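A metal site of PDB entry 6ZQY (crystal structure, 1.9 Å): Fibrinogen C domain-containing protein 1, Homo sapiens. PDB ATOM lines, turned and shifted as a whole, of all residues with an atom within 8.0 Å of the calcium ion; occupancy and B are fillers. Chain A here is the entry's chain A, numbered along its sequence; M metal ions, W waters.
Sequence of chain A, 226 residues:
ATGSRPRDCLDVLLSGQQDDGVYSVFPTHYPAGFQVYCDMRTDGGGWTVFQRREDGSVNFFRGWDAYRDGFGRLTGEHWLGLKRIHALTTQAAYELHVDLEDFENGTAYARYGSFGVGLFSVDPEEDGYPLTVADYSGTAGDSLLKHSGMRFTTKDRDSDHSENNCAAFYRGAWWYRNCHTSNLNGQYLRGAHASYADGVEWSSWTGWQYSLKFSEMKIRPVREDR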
ATOM      1  N   THR A 153     -24.796 -30.602  22.391  1.00  0.00           N
ATOM      2  CA  THR A 153     -25.493 -29.999  21.229  1.00  0.00           C
ATOM      3  C   THR A 153     -24.523 -29.905  20.044  1.00  0.00           C
ATOM      4  O   THR A 153     -23.384 -29.415  20.223  1.00  0.00           O
ATOM      5  CB  THR A 153     -26.110 -28.646  21.604  1.00  0.00           C
ATOM      6  OG1 THR A 153     -27.278 -28.903  22.367  1.00  0.00           O
ATOM      7  CG2 THR A 153     -26.465 -27.798  20.405  1.00  0.00           C
ATOM      8  N   ARG A 157     -28.383 -31.249  16.019  1.00  0.00           N
ATOM      9  CA  ARG A 157     -29.114 -31.815  17.179  1.00  0.00           C
ATOM     10  C   ARG A 157     -29.026 -30.853  18.372  1.00  0.00           C
ATOM     11  O   ARG A 157     -28.008 -30.877  19.111  1.00  0.00           O
ATOM     12  CB  ARG A 157     -28.599 -33.206  17.546  1.00  0.00           C
ATOM     13  CG  ARG A 157     -29.573 -34.023  18.389  1.00  0.00           C
ATOM     14  CD  ARG A 157     -28.969 -35.337  18.809  1.00  0.00           C
ATOM     15  NE  ARG A 157     -29.903 -36.257  19.451  1.00  0.00           N
ATOM     16  CZ  ARG A 157     -30.206 -36.282  20.751  1.00  0.00           C
ATOM     17  NH1 ARG A 157     -29.679 -35.402  21.595  1.00  0.00           N
ATOM     18  NH2 ARG A 157     -31.063 -37.180  21.205  1.00  0.00           N
ATOM     19  N   ASP A 158     -30.089 -30.079  18.575  1.00  0.00           N
ATOM     20  CA  ASP A 158     -30.160 -28.954  19.543  1.00  0.00           C
ATOM     21  C   ASP A 158     -30.824 -29.434  20.828  1.00  0.00           C
ATOM     22  O   ASP A 158     -32.041 -29.707  20.806  1.00  0.00           O
ATOM     23  CB  ASP A 158     -30.921 -27.798  18.904  1.00  0.00           C
ATOM     24  CG  ASP A 158     -31.007 -26.554  19.766  1.00  0.00           C
ATOM     25  OD1 ASP A 158     -30.809 -26.662  20.992  1.00  0.00           O
ATOM     26  OD2 ASP A 158     -31.298 -25.480  19.188  1.00  0.00           O
ATOM     27  N   SER A 159     -30.049 -29.524  21.920  1.00  0.00           N
ATOM     28  CA  SER A 159     -30.525 -29.839  23.295  1.00  0.00           C
ATOM     29  C   SER A 159     -30.080 -28.745  24.266  1.00  0.00           C
ATOM     30  O   SER A 159     -29.971 -29.026  25.467  1.00  0.00           O
ATOM     31  CB  SER A 159     -30.034 -31.191  23.748  1.00  0.00           C
ATOM     32  OG  SER A 159     -30.357 -32.197  22.810  1.00  0.00           O
ATOM     33  N   ASP A 160     -29.823 -27.524  23.768  1.00  0.00           N
ATOM     34  CA  ASP A 160     -29.299 -26.406  24.597  1.00  0.00           C
ATOM     35  C   ASP A 160     -30.477 -25.624  25.170  1.00  0.00           C
ATOM     36  O   ASP A 160     -31.640 -25.997  24.891  1.00  0.00           O
ATOM     37  CB  ASP A 160     -28.319 -25.534  23.797  1.00  0.00           C
ATOM     38  CG  ASP A 160     -28.932 -24.821  22.594  1.00  0.00           C
ATOM     39  OD1 ASP A 160     -30.024 -24.260  22.750  1.00  0.00           O
ATOM     40  OD2 ASP A 160     -28.312 -24.852  21.522  1.00  0.00           O
ATOM     41  N   HIS A 161     -30.185 -24.573  25.953  1.00  0.00           N
ATOM     42  CA  HIS A 161     -31.174 -23.692  26.621  1.00  0.00           C
ATOM     43  C   HIS A 161     -31.257 -22.340  25.898  1.00  0.00           C
ATOM     44  O   HIS A 161     -31.692 -21.359  26.522  1.00  0.00           O
ATOM     45  CB  HIS A 161     -30.810 -23.533  28.103  1.00  0.00           C
ATOM     46  CG  HIS A 161     -31.097 -24.740  28.935  1.00  0.00           C
ATOM     47  ND1 HIS A 161     -30.877 -24.761  30.293  1.00  0.00           N
ATOM     48  CD2 HIS A 161     -31.619 -25.948  28.622  1.00  0.00           C
ATOM     49  CE1 HIS A 161     -31.226 -25.940  30.781  1.00  0.00           C
ATOM     50  NE2 HIS A 161     -31.686 -26.681  29.779  1.00  0.00           N
ATOM     51  N   SER A 162     -30.874 -22.303  24.618  1.00  0.00           N
ATOM     52  CA  SER A 162     -31.012 -21.101  23.752  1.00  0.00           C
ATOM     53  C   SER A 162     -32.191 -21.289  22.799  1.00  0.00           C
ATOM     54  O   SER A 162     -32.483 -22.456  22.451  1.00  0.00           O
ATOM     55  CB  SER A 162     -29.748 -20.833  22.995  1.00  0.00           C
ATOM     56  OG  SER A 162     -29.952 -19.784  22.073  1.00  0.00           O
ATOM     57  N   GLU A 163     -32.824 -20.202  22.384  1.00  0.00           N
ATOM     58  CA  GLU A 163     -33.940 -20.197  21.401  1.00  0.00           C
ATOM     59  C   GLU A 163     -33.390 -20.561  20.014  1.00  0.00           C
ATOM     60  O   GLU A 163     -34.182 -21.008  19.168  1.00  0.00           O
ATOM     61  CB  GLU A 163     -34.640 -18.838  21.383  1.00  0.00           C
ATOM     62  CG  GLU A 163     -35.383 -18.522  22.676  1.00  0.00           C
ATOM     63  CD  GLU A 163     -36.159 -17.211  22.666  1.00  0.00           C
ATOM     64  OE1 GLU A 163     -35.700 -16.254  21.991  1.00  0.00           O
ATOM     65  OE2 GLU A 163     -37.218 -17.149  23.325  1.00  0.00           O
ATOM     66  N   ASN A 164     -32.081 -20.375  19.790  1.00  0.00           N
ATOM     67  CA  ASN A 164     -31.383 -20.818  18.553  1.00  0.00           C
ATOM     68  C   ASN A 164     -30.488 -22.018  18.899  1.00  0.00           C
ATOM     69  O   ASN A 164     -30.545 -22.523  20.037  1.00  0.00           O
ATOM     70  CB  ASN A 164     -30.625 -19.660  17.888  1.00  0.00           C
ATOM     71  CG  ASN A 164     -29.618 -18.993  18.798  1.00  0.00           C
ATOM     72  OD1 ASN A 164     -28.715 -19.632  19.316  1.00  0.00           O
ATOM     73  ND2 ASN A 164     -29.780 -17.689  18.977  1.00  0.00           N
ATOM     74  N   ASN A 165     -29.714 -22.480  17.910  1.00  0.00           N
ATOM     75  CA  ASN A 165     -28.761 -23.613  18.061  1.00  0.00           C
ATOM     76  C   ASN A 165     -27.389 -23.023  18.391  1.00  0.00           C
ATOM     77  O   ASN A 165     -26.783 -22.418  17.496  1.00  0.00           O
ATOM     78  CB  ASN A 165     -28.749 -24.474  16.788  1.00  0.00           C
ATOM     79  CG  ASN A 165     -27.846 -25.685  16.931  1.00  0.00           C
ATOM     80  OD1 ASN A 165     -26.730 -25.576  17.416  1.00  0.00           O
ATOM     81  ND2 ASN A 165     -28.336 -26.840  16.495  1.00  0.00           N
ATOM     82  N   CYS A 166     -26.932 -23.205  19.630  1.00  0.00           N
ATOM     83  CA  CYS A 166     -25.633 -22.666  20.137  1.00  0.00           C
ATOM     84  C   CYS A 166     -24.465 -23.182  19.281  1.00  0.00           C
ATOM     85  O   CYS A 166     -23.532 -22.401  19.038  1.00  0.00           O
ATOM     86  CB  CYS A 166     -25.375 -23.030  21.594  1.00  0.00           C
ATOM     87  SG  CYS A 166     -26.482 -22.200  22.758  1.00  0.00           S
ATOM     88  N   ALA A 167     -24.509 -24.452  18.868  1.00  0.00           N
ATOM     89  CA  ALA A 167     -23.452 -25.103  18.055  1.00  0.00           C
ATOM     90  C   ALA A 167     -23.345 -24.399  16.700  1.00  0.00           C
ATOM     91  O   ALA A 167     -22.212 -24.130  16.259  1.00  0.00           O
ATOM     92  CB  ALA A 167     -23.747 -26.580  17.900  1.00  0.00           C
ATOM     93  N   TYR A 176     -23.702 -27.073  25.592  1.00  0.00           N
ATOM     94  CA  TYR A 176     -24.089 -25.643  25.555  1.00  0.00           C
ATOM     95  C   TYR A 176     -25.262 -25.403  26.493  1.00  0.00           C
ATOM     96  O   TYR A 176     -26.182 -26.259  26.568  1.00  0.00           O
ATOM     97  CB  TYR A 176     -24.461 -25.205  24.132  1.00  0.00           C
ATOM     98  CG  TYR A 176     -23.302 -25.084  23.168  1.00  0.00           C
ATOM     99  CD1 TYR A 176     -22.333 -24.107  23.311  1.00  0.00           C
ATOM    100  CD2 TYR A 176     -23.219 -25.923  22.073  1.00  0.00           C
ATOM    101  CE1 TYR A 176     -21.283 -23.985  22.409  1.00  0.00           C
ATOM    102  CE2 TYR A 176     -22.184 -25.814  21.158  1.00  0.00           C
ATOM    103  CZ  TYR A 176     -21.218 -24.838  21.317  1.00  0.00           C
ATOM    104  OH  TYR A 176     -20.215 -24.747  20.398  1.00  0.00           O
ATOM    105  N   ARG A 177     -25.232 -24.258  27.188  1.00  0.00           N
ATOM    106  CA  ARG A 177     -26.380 -23.744  27.993  1.00  0.00           C
ATOM    107  C   ARG A 177     -27.024 -22.611  27.188  1.00  0.00           C
ATOM    108  O   ARG A 177     -27.891 -22.912  26.358  1.00  0.00           O
ATOM    109  CB  ARG A 177     -25.911 -23.348  29.399  1.00  0.00           C
ATOM    110  CG  ARG A 177     -27.044 -22.885  30.305  1.00  0.00           C
ATOM    111  CD  ARG A 177     -26.598 -22.535  31.707  1.00  0.00           C
ATOM    112  NE  ARG A 177     -25.975 -23.655  32.399  1.00  0.00           N
ATOM    113  CZ  ARG A 177     -26.616 -24.599  33.100  1.00  0.00           C
ATOM    114  NH1 ARG A 177     -27.937 -24.575  33.214  1.00  0.00           N
ATOM    115  NH2 ARG A 177     -25.936 -25.568  33.685  1.00  0.00           N
ATOM    116  N   ASN A 178     -26.560 -21.367  27.378  1.00  0.00           N
ATOM    117  CA  ASN A 178     -27.110 -20.177  26.666  1.00  0.00           C
ATOM    118  C   ASN A 178     -26.065 -19.067  26.622  1.00  0.00           C
ATOM    119  O   ASN A 178     -26.298 -17.988  27.173  1.00  0.00           O
ATOM    120  CB  ASN A 178     -28.411 -19.741  27.347  1.00  0.00           C
ATOM    121  CG  ASN A 178     -29.158 -18.666  26.581  1.00  0.00           C
ATOM    122  OD1 ASN A 178     -29.165 -18.665  25.353  1.00  0.00           O
ATOM    123  ND2 ASN A 178     -29.791 -17.751  27.303  1.00  0.00           N
ATOM    124  N   CYS A 179     -24.909 -19.298  25.972  1.00  0.00           N
ATOM    125  CA  CYS A 179     -24.553 -20.533  25.294  1.00  0.00           C
ATOM    126  C   CYS A 179     -23.319 -21.180  25.944  1.00  0.00           C
ATOM    127  O   CYS A 179     -23.391 -22.380  26.256  1.00  0.00           O
ATOM    128  CB  CYS A 179     -24.305 -20.308  23.803  1.00  0.00           C
ATOM    129  SG  CYS A 179     -25.813 -20.245  22.797  1.00  0.00           S
HETATM  130 CA    CA M   1     -31.714 -24.312  21.191  1.00  0.00          CA
HETATM  131  O   HOH W   1     -33.865 -24.054  20.116  1.00  0.00           O
HETATM  132  O   HOH W   2     -33.082 -25.463  22.743  1.00  0.00           O
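The side-chain hydroxyl (OG) of Ser 162 is in hydrogen-bond range of the side-chain amide oxygen (OD1) of Asn 164 (3.0 Å). The side-chain hydroxyl (OG1) of Thr 153 is in hydrogen-bond range of the backbone NH (N) of Asp 160 (3.2 Å). The side-chain sulfur (SG) of Cys 166 is disulfide-bonded to the side-chain sulfur (SG) of Cys 179 (2.1 Å). The backbone NH of Cys 166 is in hydrogen-bond range of the side-chain carboxylate of Asp 160 (2.9 Å).
The calcium ion is bound by OD1 of Asp 160, OD2 of Asp 158, water W2, O of Ser 162, water W1, O of Asn 164 and OD1 of Asp 158.
Of the 16 residues printed, 4 come within 4 Å of the calcium ion. The nearest printed residue that does not touch the calcium ion is Asn 165 (4.3 Å).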
